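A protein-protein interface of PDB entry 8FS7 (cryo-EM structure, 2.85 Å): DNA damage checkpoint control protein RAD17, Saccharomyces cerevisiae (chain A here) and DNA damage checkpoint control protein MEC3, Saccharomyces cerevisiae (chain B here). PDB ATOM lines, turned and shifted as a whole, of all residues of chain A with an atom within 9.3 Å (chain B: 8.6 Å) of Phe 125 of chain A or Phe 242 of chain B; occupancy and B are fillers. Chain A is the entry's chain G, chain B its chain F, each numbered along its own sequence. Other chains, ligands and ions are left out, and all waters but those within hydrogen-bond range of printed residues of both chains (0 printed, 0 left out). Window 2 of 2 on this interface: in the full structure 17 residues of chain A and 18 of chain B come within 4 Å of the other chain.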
ATOM      1  N   ASN A  99     -23.754 -14.857  34.986  1.00  0.00           N
ATOM      2  CA  ASN A  99     -24.802 -14.528  34.014  1.00  0.00           C
ATOM      3  C   ASN A  99     -26.100 -14.132  34.727  1.00  0.00           C
ATOM      4  O   ASN A  99     -27.112 -14.836  34.695  1.00  0.00           O
ATOM      5  CB  ASN A  99     -25.023 -15.685  33.031  1.00  0.00           C
ATOM      6  CG  ASN A  99     -23.757 -16.059  32.280  1.00  0.00           C
ATOM      7  OD1 ASN A  99     -22.676 -15.546  32.568  1.00  0.00           O
ATOM      8  ND2 ASN A  99     -23.889 -16.951  31.306  1.00  0.00           N
ATOM      9  N   ASP A 102     -29.840 -15.110  34.181  1.00  0.00           N
ATOM     10  CA  ASP A 102     -30.310 -16.450  34.516  1.00  0.00           C
ATOM     11  C   ASP A 102     -29.569 -16.932  35.761  1.00  0.00           C
ATOM     12  O   ASP A 102     -28.469 -17.483  35.696  1.00  0.00           O
ATOM     13  CB  ASP A 102     -30.110 -17.390  33.337  1.00  0.00           C
ATOM     14  CG  ASP A 102     -31.157 -18.468  33.285  1.00  0.00           C
ATOM     15  OD1 ASP A 102     -31.527 -18.984  34.359  1.00  0.00           O
ATOM     16  OD2 ASP A 102     -31.629 -18.778  32.173  1.00  0.00           O
ATOM     17  N   ILE A 103     -30.197 -16.717  36.917  1.00  0.00           N
ATOM     18  CA  ILE A 103     -29.583 -17.075  38.192  1.00  0.00           C
ATOM     19  C   ILE A 103     -29.730 -18.572  38.431  1.00  0.00           C
ATOM     20  O   ILE A 103     -30.809 -19.146  38.238  1.00  0.00           O
ATOM     21  CB  ILE A 103     -30.211 -16.255  39.330  1.00  0.00           C
ATOM     22  CG1 ILE A 103     -29.685 -14.817  39.313  1.00  0.00           C
ATOM     23  CG2 ILE A 103     -29.938 -16.894  40.685  1.00  0.00           C
ATOM     24  CD1 ILE A 103     -28.222 -14.698  38.940  1.00  0.00           C
ATOM     25  N   VAL A 104     -28.639 -19.213  38.847  1.00  0.00           N
ATOM     26  CA  VAL A 104     -28.659 -20.624  39.220  1.00  0.00           C
ATOM     27  C   VAL A 104     -29.502 -20.794  40.476  1.00  0.00           C
ATOM     28  O   VAL A 104     -29.304 -20.085  41.471  1.00  0.00           O
ATOM     29  CB  VAL A 104     -27.231 -21.148  39.442  1.00  0.00           C
ATOM     30  CG1 VAL A 104     -27.247 -22.637  39.761  1.00  0.00           C
ATOM     31  CG2 VAL A 104     -26.362 -20.860  38.232  1.00  0.00           C
ATOM     32  N   PHE A 121     -29.195 -28.155  40.756  1.00  0.00           N
ATOM     33  CA  PHE A 121     -28.922 -26.810  40.273  1.00  0.00           C
ATOM     34  C   PHE A 121     -29.639 -26.610  38.947  1.00  0.00           C
ATOM     35  O   PHE A 121     -29.462 -27.403  38.016  1.00  0.00           O
ATOM     36  CB  PHE A 121     -27.419 -26.577  40.108  1.00  0.00           C
ATOM     37  CG  PHE A 121     -26.677 -26.503  41.410  1.00  0.00           C
ATOM     38  CD1 PHE A 121     -26.701 -25.346  42.170  1.00  0.00           C
ATOM     39  CD2 PHE A 121     -25.963 -27.594  41.879  1.00  0.00           C
ATOM     40  CE1 PHE A 121     -26.022 -25.275  43.370  1.00  0.00           C
ATOM     41  CE2 PHE A 121     -25.282 -27.529  43.080  1.00  0.00           C
ATOM     42  CZ  PHE A 121     -25.314 -26.368  43.826  1.00  0.00           C
ATOM     43  N   GLU A 122     -30.444 -25.554  38.862  1.00  0.00           N
ATOM     44  CA  GLU A 122     -31.236 -25.263  37.677  1.00  0.00           C
ATOM     45  C   GLU A 122     -30.834 -23.913  37.106  1.00  0.00           C
ATOM     46  O   GLU A 122     -30.789 -22.914  37.830  1.00  0.00           O
ATOM     47  CB  GLU A 122     -32.735 -25.277  37.993  1.00  0.00           C
ATOM     48  CG  GLU A 122     -33.182 -26.474  38.810  1.00  0.00           C
ATOM     49  CD  GLU A 122     -33.760 -27.578  37.948  1.00  0.00           C
ATOM     50  OE1 GLU A 122     -34.781 -27.332  37.270  1.00  0.00           O
ATOM     51  OE2 GLU A 122     -33.192 -28.689  37.945  1.00  0.00           O
ATOM     52  N   ASP A 123     -30.550 -23.892  35.804  1.00  0.00           N
ATOM     53  CA  ASP A 123     -30.224 -22.670  35.089  1.00  0.00           C
ATOM     54  C   ASP A 123     -31.189 -22.390  33.944  1.00  0.00           C
ATOM     55  O   ASP A 123     -30.941 -21.465  33.167  1.00  0.00           O
ATOM     56  CB  ASP A 123     -28.781 -22.745  34.546  1.00  0.00           C
ATOM     57  CG  ASP A 123     -28.145 -21.370  34.327  1.00  0.00           C
ATOM     58  OD1 ASP A 123     -28.381 -20.732  33.280  1.00  0.00           O
ATOM     59  OD2 ASP A 123     -27.377 -20.937  35.208  1.00  0.00           O
ATOM     60  N   SER A 124     -32.238 -23.208  33.775  1.00  0.00           N
ATOM     61  CA  SER A 124     -33.230 -23.101  32.701  1.00  0.00           C
ATOM     62  C   SER A 124     -32.616 -23.453  31.347  1.00  0.00           C
ATOM     63  O   SER A 124     -33.325 -23.561  30.342  1.00  0.00           O
ATOM     64  CB  SER A 124     -33.868 -21.707  32.660  1.00  0.00           C
ATOM     65  OG  SER A 124     -34.543 -21.420  33.873  1.00  0.00           O
ATOM     66  N   PHE A 125     -31.301 -23.647  31.330  1.00  0.00           N
ATOM     67  CA  PHE A 125     -30.530 -24.093  30.181  1.00  0.00           C
ATOM     68  C   PHE A 125     -29.633 -25.272  30.512  1.00  0.00           C
ATOM     69  O   PHE A 125     -29.357 -26.094  29.635  1.00  0.00           O
ATOM     70  CB  PHE A 125     -29.657 -22.944  29.651  1.00  0.00           C
ATOM     71  CG  PHE A 125     -30.252 -22.203  28.486  1.00  0.00           C
ATOM     72  CD1 PHE A 125     -31.560 -22.426  28.089  1.00  0.00           C
ATOM     73  CD2 PHE A 125     -29.491 -21.285  27.779  1.00  0.00           C
ATOM     74  CE1 PHE A 125     -32.101 -21.740  27.016  1.00  0.00           C
ATOM     75  CE2 PHE A 125     -30.027 -20.595  26.710  1.00  0.00           C
ATOM     76  CZ  PHE A 125     -31.331 -20.824  26.327  1.00  0.00           C
ATOM     77  N   ILE A 126     -29.171 -25.367  31.759  1.00  0.00           N
ATOM     78  CA  ILE A 126     -28.315 -26.443  32.240  1.00  0.00           C
ATOM     79  C   ILE A 126     -28.942 -27.005  33.507  1.00  0.00           C
ATOM     80  O   ILE A 126     -29.256 -26.250  34.434  1.00  0.00           O
ATOM     81  CB  ILE A 126     -26.885 -25.943  32.525  1.00  0.00           C
ATOM     82  CG1 ILE A 126     -26.300 -25.251  31.292  1.00  0.00           C
ATOM     83  CG2 ILE A 126     -25.992 -27.088  32.989  1.00  0.00           C
ATOM     84  CD1 ILE A 126     -25.125 -24.357  31.594  1.00  0.00           C
ATOM     85  N   SER A 127     -29.130 -28.321  33.549  1.00  0.00           N
ATOM     86  CA  SER A 127     -29.653 -29.002  34.729  1.00  0.00           C
ATOM     87  C   SER A 127     -28.573 -29.922  35.273  1.00  0.00           C
ATOM     88  O   SER A 127     -28.063 -30.782  34.548  1.00  0.00           O
ATOM     89  CB  SER A 127     -30.922 -29.791  34.400  1.00  0.00           C
ATOM     90  OG  SER A 127     -31.961 -28.931  33.965  1.00  0.00           O
ATOM     91  N   GLU A 128     -28.223 -29.738  36.543  1.00  0.00           N
ATOM     92  CA  GLU A 128     -27.194 -30.535  37.200  1.00  0.00           C
ATOM     93  C   GLU A 128     -27.757 -31.098  38.496  1.00  0.00           C
ATOM     94  O   GLU A 128     -28.261 -30.345  39.337  1.00  0.00           O
ATOM     95  CB  GLU A 128     -25.942 -29.700  37.472  1.00  0.00           C
ATOM     96  CG  GLU A 128     -25.020 -30.290  38.525  1.00  0.00           C
ATOM     97  CD  GLU A 128     -23.806 -29.423  38.784  1.00  0.00           C
ATOM     98  OE1 GLU A 128     -23.694 -28.352  38.152  1.00  0.00           O
ATOM     99  OE2 GLU A 128     -22.962 -29.810  39.619  1.00  0.00           O
ATOM    100  N   LEU B 235     -21.827 -28.154  18.145  1.00  0.00           N
ATOM    101  CA  LEU B 235     -21.898 -27.327  19.337  1.00  0.00           C
ATOM    102  C   LEU B 235     -22.186 -25.880  18.944  1.00  0.00           C
ATOM    103  O   LEU B 235     -21.705 -25.412  17.903  1.00  0.00           O
ATOM    104  CB  LEU B 235     -20.591 -27.420  20.127  1.00  0.00           C
ATOM    105  CG  LEU B 235     -20.037 -28.832  20.363  1.00  0.00           C
ATOM    106  CD1 LEU B 235     -18.854 -28.805  21.320  1.00  0.00           C
ATOM    107  CD2 LEU B 235     -21.110 -29.789  20.869  1.00  0.00           C
ATOM    108  N   PRO B 236     -22.973 -25.154  19.733  1.00  0.00           N
ATOM    109  CA  PRO B 236     -23.348 -23.783  19.362  1.00  0.00           C
ATOM    110  C   PRO B 236     -22.136 -22.871  19.330  1.00  0.00           C
ATOM    111  O   PRO B 236     -21.212 -23.022  20.143  1.00  0.00           O
ATOM    112  CB  PRO B 236     -24.328 -23.369  20.472  1.00  0.00           C
ATOM    113  CG  PRO B 236     -24.762 -24.656  21.113  1.00  0.00           C
ATOM    114  CD  PRO B 236     -23.581 -25.563  21.008  1.00  0.00           C
ATOM    115  N   PRO B 237     -22.094 -21.923  18.393  1.00  0.00           N
ATOM    116  CA  PRO B 237     -20.988 -20.959  18.372  1.00  0.00           C
ATOM    117  C   PRO B 237     -20.999 -20.087  19.618  1.00  0.00           C
ATOM    118  O   PRO B 237     -22.057 -19.734  20.141  1.00  0.00           O
ATOM    119  CB  PRO B 237     -21.255 -20.140  17.104  1.00  0.00           C
ATOM    120  CG  PRO B 237     -22.717 -20.310  16.841  1.00  0.00           C
ATOM    121  CD  PRO B 237     -23.052 -21.697  17.299  1.00  0.00           C
ATOM    122  N   ILE B 238     -19.800 -19.733  20.089  1.00  0.00           N
ATOM    123  CA  ILE B 238     -19.689 -18.965  21.323  1.00  0.00           C
ATOM    124  C   ILE B 238     -20.142 -17.521  21.144  1.00  0.00           C
ATOM    125  O   ILE B 238     -20.411 -16.835  22.136  1.00  0.00           O
ATOM    126  CB  ILE B 238     -18.248 -19.031  21.869  1.00  0.00           C
ATOM    127  CG1 ILE B 238     -18.262 -18.993  23.400  1.00  0.00           C
ATOM    128  CG2 ILE B 238     -17.394 -17.905  21.298  1.00  0.00           C
ATOM    129  CD1 ILE B 238     -16.892 -18.892  24.026  1.00  0.00           C
ATOM    130  N   SER B 239     -20.240 -17.038  19.904  1.00  0.00           N
ATOM    131  CA  SER B 239     -20.722 -15.683  19.667  1.00  0.00           C
ATOM    132  C   SER B 239     -22.239 -15.581  19.735  1.00  0.00           C
ATOM    133  O   SER B 239     -22.768 -14.468  19.818  1.00  0.00           O
ATOM    134  CB  SER B 239     -20.234 -15.177  18.308  1.00  0.00           C
ATOM    135  OG  SER B 239     -20.725 -15.989  17.256  1.00  0.00           O
ATOM    136  N   GLY B 240     -22.947 -16.709  19.702  1.00  0.00           N
ATOM    137  CA  GLY B 240     -24.391 -16.702  19.753  1.00  0.00           C
ATOM    138  C   GLY B 240     -24.926 -16.517  21.160  1.00  0.00           C
ATOM    139  O   GLY B 240     -24.187 -16.389  22.137  1.00  0.00           O
ATOM    140  N   GLU B 241     -26.258 -16.490  21.250  1.00  0.00           N
ATOM    141  CA  GLU B 241     -26.915 -16.348  22.547  1.00  0.00           C
ATOM    142  C   GLU B 241     -26.622 -17.539  23.450  1.00  0.00           C
ATOM    143  O   GLU B 241     -26.355 -17.371  24.646  1.00  0.00           O
ATOM    144  CB  GLU B 241     -28.421 -16.174  22.351  1.00  0.00           C
ATOM    145  CG  GLU B 241     -29.269 -16.440  23.593  1.00  0.00           C
ATOM    146  CD  GLU B 241     -29.238 -15.298  24.596  1.00  0.00           C
ATOM    147  OE1 GLU B 241     -28.160 -15.015  25.160  1.00  0.00           O
ATOM    148  OE2 GLU B 241     -30.300 -14.680  24.819  1.00  0.00           O
ATOM    149  N   PHE B 242     -26.660 -18.749  22.896  1.00  0.00           N
ATOM    150  CA  PHE B 242     -26.437 -19.963  23.670  1.00  0.00           C
ATOM    151  C   PHE B 242     -24.963 -20.300  23.842  1.00  0.00           C
ATOM    152  O   PHE B 242     -24.649 -21.284  24.520  1.00  0.00           O
ATOM    153  CB  PHE B 242     -27.158 -21.142  23.010  1.00  0.00           C
ATOM    154  CG  PHE B 242     -28.496 -20.786  22.429  1.00  0.00           C
ATOM    155  CD1 PHE B 242     -29.584 -20.545  23.252  1.00  0.00           C
ATOM    156  CD2 PHE B 242     -28.666 -20.691  21.057  1.00  0.00           C
ATOM    157  CE1 PHE B 242     -30.815 -20.217  22.718  1.00  0.00           C
ATOM    158  CE2 PHE B 242     -29.895 -20.363  20.518  1.00  0.00           C
ATOM    159  CZ  PHE B 242     -30.972 -20.125  21.350  1.00  0.00           C
ATOM    160  N   GLY B 243     -24.058 -19.519  23.248  1.00  0.00           N
ATOM    161  CA  GLY B 243     -22.644 -19.860  23.311  1.00  0.00           C
ATOM    162  C   GLY B 243     -22.071 -19.770  24.713  1.00  0.00           C
ATOM    163  O   GLY B 243     -21.333 -20.656  25.152  1.00  0.00           O
ATOM    164  N   SER B 244     -22.397 -18.694  25.434  1.00  0.00           N
ATOM    165  CA  SER B 244     -21.911 -18.548  26.804  1.00  0.00           C
ATOM    166  C   SER B 244     -22.497 -19.621  27.714  1.00  0.00           C
ATOM    167  O   SER B 244     -21.795 -20.166  28.576  1.00  0.00           O
ATOM    168  CB  SER B 244     -22.240 -17.153  27.332  1.00  0.00           C
ATOM    169  OG  SER B 244     -23.637 -16.916  27.310  1.00  0.00           O
ATOM    170  N   ALA B 245     -23.781 -19.937  27.533  1.00  0.00           N
ATOM    171  CA  ALA B 245     -24.405 -20.994  28.323  1.00  0.00           C
ATOM    172  C   ALA B 245     -23.756 -22.343  28.045  1.00  0.00           C
ATOM    173  O   ALA B 245     -23.526 -23.132  28.969  1.00  0.00           O
ATOM    174  CB  ALA B 245     -25.904 -21.047  28.039  1.00  0.00           C
ATOM    175  N   PHE B 246     -23.443 -22.628  26.778  1.00  0.00           N
ATOM    176  CA  PHE B 246     -22.787 -23.890  26.457  1.00  0.00           C
ATOM    177  C   PHE B 246     -21.360 -23.935  26.989  1.00  0.00           C
ATOM    178  O   PHE B 246     -20.895 -24.997  27.409  1.00  0.00           O
ATOM    179  CB  PHE B 246     -22.797 -24.132  24.950  1.00  0.00           C
ATOM    180  CG  PHE B 246     -22.458 -25.541  24.571  1.00  0.00           C
ATOM    181  CD1 PHE B 246     -23.382 -26.557  24.745  1.00  0.00           C
ATOM    182  CD2 PHE B 246     -21.210 -25.856  24.063  1.00  0.00           C
ATOM    183  CE1 PHE B 246     -23.074 -27.859  24.406  1.00  0.00           C
ATOM    184  CE2 PHE B 246     -20.895 -27.155  23.724  1.00  0.00           C
ATOM    185  CZ  PHE B 246     -21.829 -28.159  23.897  1.00  0.00           C
ATOM    186  N   HIS B 247     -20.652 -22.803  26.974  1.00  0.00           N
ATOM    187  CA  HIS B 247     -19.320 -22.757  27.571  1.00  0.00           C
ATOM    188  C   HIS B 247     -19.388 -23.029  29.069  1.00  0.00           C
ATOM    189  O   HIS B 247     -18.561 -23.771  29.616  1.00  0.00           O
ATOM    190  CB  HIS B 247     -18.672 -21.401  27.293  1.00  0.00           C
ATOM    191  CG  HIS B 247     -17.190 -21.383  27.506  1.00  0.00           C
ATOM    192  ND1 HIS B 247     -16.356 -22.371  27.027  1.00  0.00           N
ATOM    193  CD2 HIS B 247     -16.391 -20.489  28.135  1.00  0.00           C
ATOM    194  CE1 HIS B 247     -15.108 -22.089  27.358  1.00  0.00           C
ATOM    195  NE2 HIS B 247     -15.102 -20.953  28.030  1.00  0.00           N
ATOM    196  N   GLY B 248     -20.374 -22.437  29.747  1.00  0.00           N
ATOM    197  CA  GLY B 248     -20.582 -22.744  31.153  1.00  0.00           C
ATOM    198  C   GLY B 248     -20.915 -24.206  31.383  1.00  0.00           C
ATOM    199  O   GLY B 248     -20.451 -24.811  32.350  1.00  0.00           O
ATOM    200  N   PHE B 249     -21.717 -24.792  30.492  1.00  0.00           N
ATOM    201  CA  PHE B 249     -22.026 -26.216  30.590  1.00  0.00           C
ATOM    202  C   PHE B 249     -20.771 -27.069  30.441  1.00  0.00           C
ATOM    203  O   PHE B 249     -20.597 -28.060  31.161  1.00  0.00           O
ATOM    204  CB  PHE B 249     -23.059 -26.599  29.530  1.00  0.00           C
ATOM    205  CG  PHE B 249     -23.187 -28.079  29.319  1.00  0.00           C
ATOM    206  CD1 PHE B 249     -23.737 -28.888  30.297  1.00  0.00           C
ATOM    207  CD2 PHE B 249     -22.749 -28.662  28.140  1.00  0.00           C
ATOM    208  CE1 PHE B 249     -23.852 -30.251  30.104  1.00  0.00           C
ATOM    209  CE2 PHE B 249     -22.861 -30.023  27.941  1.00  0.00           C
ATOM    210  CZ  PHE B 249     -23.412 -30.819  28.924  1.00  0.00           C
ATOM    211  N   ARG B 252     -18.648 -26.692  33.554  1.00  0.00           N
ATOM    212  CA  ARG B 252     -19.322 -27.039  34.800  1.00  0.00           C
ATOM    213  C   ARG B 252     -18.686 -28.232  35.504  1.00  0.00           C
ATOM    214  O   ARG B 252     -18.800 -28.345  36.729  1.00  0.00           O
ATOM    215  CB  ARG B 252     -20.800 -27.324  34.522  1.00  0.00           C
ATOM    216  CG  ARG B 252     -21.694 -27.234  35.744  1.00  0.00           C
ATOM    217  CD  ARG B 252     -21.660 -25.838  36.342  1.00  0.00           C
ATOM    218  NE  ARG B 252     -22.295 -24.851  35.475  1.00  0.00           N
ATOM    219  CZ  ARG B 252     -23.567 -24.489  35.560  1.00  0.00           C
ATOM    220  NH1 ARG B 252     -24.379 -25.021  36.460  1.00  0.00           N
ATOM    221  NH2 ARG B 252     -24.038 -23.571  34.722  1.00  0.00           N
ATOM    222  N   LEU B 281     -26.670 -33.420  25.396  1.00  0.00           N
ATOM    223  CA  LEU B 281     -25.315 -33.742  25.826  1.00  0.00           C
ATOM    224  C   LEU B 281     -25.308 -33.767  27.348  1.00  0.00           C
ATOM    225  O   LEU B 281     -25.639 -32.764  27.987  1.00  0.00           O
ATOM    226  CB  LEU B 281     -24.305 -32.726  25.291  1.00  0.00           C
ATOM    227  CG  LEU B 281     -23.402 -33.212  24.155  1.00  0.00           C
ATOM    228  CD1 LEU B 281     -22.683 -32.034  23.512  1.00  0.00           C
ATOM    229  CD2 LEU B 281     -22.417 -34.260  24.646  1.00  0.00           C
ATOM    230  N   ILE B 294     -24.811 -33.411  35.052  1.00  0.00           N
ATOM    231  CA  ILE B 294     -24.869 -32.185  34.263  1.00  0.00           C
ATOM    232  C   ILE B 294     -25.512 -32.479  32.915  1.00  0.00           C
ATOM    233  O   ILE B 294     -25.105 -33.404  32.202  1.00  0.00           O
ATOM    234  CB  ILE B 294     -23.468 -31.580  34.086  1.00  0.00           C
ATOM    235  CG1 ILE B 294     -22.644 -31.736  35.362  1.00  0.00           C
ATOM    236  CG2 ILE B 294     -23.570 -30.113  33.704  1.00  0.00           C
ATOM    237  CD1 ILE B 294     -21.243 -31.177  35.247  1.00  0.00           C
ATOM    238  N   CYS B 295     -26.523 -31.688  32.561  1.00  0.00           N
ATOM    239  CA  CYS B 295     -27.255 -31.871  31.317  1.00  0.00           C
ATOM    240  C   CYS B 295     -27.441 -30.524  30.635  1.00  0.00           C
ATOM    241  O   CYS B 295     -27.530 -29.485  31.293  1.00  0.00           O
ATOM    242  CB  CYS B 295     -28.622 -32.528  31.558  1.00  0.00           C
ATOM    243  SG  CYS B 295     -28.541 -34.181  32.283  1.00  0.00           S
ATOM    244  N   TRP B 296     -27.501 -30.553  29.305  1.00  0.00           N
ATOM    245  CA  TRP B 296     -27.681 -29.353  28.493  1.00  0.00           C
ATOM    246  C   TRP B 296     -29.115 -29.329  27.973  1.00  0.00           C
ATOM    247  O   TRP B 296     -29.494 -30.158  27.139  1.00  0.00           O
ATOM    248  CB  TRP B 296     -26.677 -29.320  27.344  1.00  0.00           C
ATOM    249  CG  TRP B 296     -26.941 -28.241  26.338  1.00  0.00           C
ATOM    250  CD1 TRP B 296     -27.391 -28.404  25.061  1.00  0.00           C
ATOM    251  CD2 TRP B 296     -26.763 -26.831  26.523  1.00  0.00           C
ATOM    252  NE1 TRP B 296     -27.508 -27.185  24.440  1.00  0.00           N
ATOM    253  CE2 TRP B 296     -27.128 -26.202  25.317  1.00  0.00           C
ATOM    254  CE3 TRP B 296     -26.332 -26.040  27.592  1.00  0.00           C
ATOM    255  CZ2 TRP B 296     -27.076 -24.820  25.149  1.00  0.00           C
ATOM    256  CZ3 TRP B 296     -26.280 -24.668  27.424  1.00  0.00           C
ATOM    257  CH2 TRP B 296     -26.650 -24.072  26.212  1.00  0.00           C
ATOM    258  N   ASN B 297     -29.908 -28.379  28.464  1.00  0.00           N
ATOM    259  CA  ASN B 297     -31.307 -28.252  28.075  1.00  0.00           C
ATOM    260  C   ASN B 297     -31.523 -27.268  26.933  1.00  0.00           C
ATOM    261  O   ASN B 297     -32.664 -27.089  26.497  1.00  0.00           O
ATOM    262  CB  ASN B 297     -32.153 -27.826  29.279  1.00  0.00           C
ATOM    263  CG  ASN B 297     -32.084 -28.819  30.420  1.00  0.00           C
ATOM    264  OD1 ASN B 297     -31.544 -28.520  31.483  1.00  0.00           O
ATOM    265  ND2 ASN B 297     -32.634 -30.009  30.205  1.00  0.00           N
ATOM    266  N   GLY B 298     -30.465 -26.628  26.442  1.00  0.00           N
ATOM    267  CA  GLY B 298     -30.590 -25.666  25.374  1.00  0.00           C
ATOM    268  C   GLY B 298     -30.686 -26.323  24.013  1.00  0.00           C
ATOM    269  O   GLY B 298     -30.580 -27.545  23.877  1.00  0.00           O
ATOM    270  N   PRO B 299     -30.892 -25.518  22.973  1.00  0.00           N
ATOM    271  CA  PRO B 299     -30.988 -26.074  21.619  1.00  0.00           C
ATOM    272  C   PRO B 299     -29.626 -26.493  21.087  1.00  0.00           C
ATOM    273  O   PRO B 299     -28.616 -25.816  21.297  1.00  0.00           O
ATOM    274  CB  PRO B 299     -31.572 -24.916  20.803  1.00  0.00           C
ATOM    275  CG  PRO B 299     -31.119 -23.691  21.523  1.00  0.00           C
ATOM    276  CD  PRO B 299     -31.011 -24.049  22.984  1.00  0.00           C
ATOM    277  N   LEU B 300     -29.611 -27.626  20.387  1.00  0.00           N
ATOM    278  CA  LEU B 300     -28.393 -28.175  19.813  1.00  0.00           C
ATOM    279  C   LEU B 300     -28.712 -28.717  18.425  1.00  0.00           C
ATOM    280  O   LEU B 300     -29.865 -29.005  18.096  1.00  0.00           O
ATOM    281  CB  LEU B 300     -27.798 -29.273  20.711  1.00  0.00           C
ATOM    282  CG  LEU B 300     -26.405 -29.820  20.397  1.00  0.00           C
ATOM    283  CD1 LEU B 300     -25.342 -28.801  20.770  1.00  0.00           C
ATOM    284  CD2 LEU B 300     -26.167 -31.135  21.112  1.00  0.00           C
ATOM    285  N   TYR B 422     -12.879 -24.777  22.405  1.00  0.00           N
ATOM    286  CA  TYR B 422     -14.229 -24.323  22.079  1.00  0.00           C
ATOM    287  C   TYR B 422     -14.349 -22.809  22.187  1.00  0.00           C
ATOM    288  O   TYR B 422     -15.059 -22.177  21.395  1.00  0.00           O
ATOM    289  CB  TYR B 422     -15.245 -25.011  22.990  1.00  0.00           C
ATOM    290  CG  TYR B 422     -16.633 -24.412  22.930  1.00  0.00           C
ATOM    291  CD1 TYR B 422     -17.475 -24.671  21.857  1.00  0.00           C
ATOM    292  CD2 TYR B 422     -17.103 -23.593  23.949  1.00  0.00           C
ATOM    293  CE1 TYR B 422     -18.744 -24.128  21.797  1.00  0.00           C
ATOM    294  CE2 TYR B 422     -18.371 -23.044  23.897  1.00  0.00           C
ATOM    295  CZ  TYR B 422     -19.186 -23.315  22.820  1.00  0.00           C
ATOM    296  OH  TYR B 422     -20.449 -22.773  22.763  1.00  0.00           O
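The side-chain carboxylate (OE1) of Glu 128 of chain A lies within salt-bridge range of the guanidinium group (NH1) of Arg 252 of chain B, at 3.8 Å.
The backbone NH (N) of Cys 295 of chain B is in hydrogen-bond range of the backbone carbonyl oxygen (O) of Ser 127 of chain A, 2.7 Å away.
The backbone carbonyl oxygen (O) of Phe 125 of chain A sits at hydrogen-bond distance from the backbone NH (N) of Asn 297 of chain B, at 2.6 Å.
The side-chain hydroxyl (OG) of Ser 127 of chain A lies within hydrogen-bond range of the side-chain amide oxygen (OD1) of Asn 297 of chain B, at 2.6 Å.
The backbone carbonyl oxygen (O) of Phe 125 of chain A lies within hydrogen-bond range of the backbone NH (N) of Gly 298 of chain B (3.4 Å).
The backbone carbonyl oxygen (O) of Leu 281 of chain B is in hydrogen-bond range of the backbone NH (N) of Trp 296 of chain B.
NE1 of Trp 296 of chain B lies within hydrogen-bond range of O of Gly 298 of chain B, at 3.1 Å.
The backbone NH (N) of Phe 121 of chain A lies within hydrogen-bond range of the backbone carbonyl oxygen (O) of Glu 128 of chain A (2.8 Å).
CE2 of Phe 125 of chain A touches CD1 of Phe 242 of chain B (3.5 Å).
CB of Ala 245 of chain B touches CD2 of Phe 125 of chain A, 3.6 Å away.
Phe 125 of chain A touches Trp 296 of chain B.
Ile 126 of chain A touches Ala 245 of chain B.
Phe 249 of chain B touches Ile 126 of chain A (N to CD1, 3.6 Å).
Arg 252 of chain B touches Ile 126 of chain A (NH2 to CD1, 3.4 Å).
Ile 126 of chain A touches Ile 294 of chain B.
Ile 126 of chain A touches Trp 296 of chain B (CG1 to CE3, 3.8 Å).
Asn 297 of chain B touches Ile 126 of chain A (OD1 to C, 3.6 Å).
Ile 294 of chain B touches Ser 127 of chain A (C to O, 3.5 Å).
Phe 125 of chain A touches just these residues of chain B: Phe 242 (3.5 Å), Ala 245 (3.6 Å), Trp 296 (3.6 Å), Asn 297 (2.6 Å) and Gly 298 (3.4 Å).
Of chain A, only Phe 125 (3.5 Å) comes within 4 Å of Phe 242 of chain B.
No residue of chain A comes within 4 Å of Gly 243 of chain B.
Ala 245 of chain B touches two residues of chain A.
Asn 297 of chain B touches three residues of chain A.
Of the printed residues of chain A, Arg 252 of chain B touches Ile 126 and Glu 128.
Of the printed residues of chain B, Ile 126 of chain A touches Ala 245 (3.3 Å), Phe 249 (3.6 Å), Arg 252 (3.4 Å), Ile 294 (3.9 Å), Cys 295 (3.3 Å), Trp 296 (3.8 Å) and Asn 297 (3.6 Å).
Printed residues of chain B within 4 Å of Ser 127 of chain A: Ile 294 (3.5 Å), Cys 295 (2.7 Å) and Asn 297 (2.6 Å).
Printed residues of chain A within 4 Å of Gly 298 of chain B: Phe 125.
Gly 248 of chain B touches none of the printed residues of chain A.
Of the 25 printed residues of chain B, 9 touch a printed residue of chain A.
Printed residues of chain B that touch a printed residue of chain A: Phe 242, Ala 245, Phe 249, Arg 252, Ile 294, Cys 295, Trp 296, Asn 297 and Gly 298.
Hydrophobic or aromatic side chains of chain B that line the printed part of chain A: Phe 242, Ala 245, Phe 249, Ile 294 and Trp 296.
Printed residues of chain A that touch a printed residue of chain B: Phe 125, Ile 126, Ser 127 and Glu 128.
Hydrophobic or aromatic side chains of chain A that line the printed part of chain B: Phe 125 and Ile 126.
Among the printed residues, 16 pairs touch across the chains.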
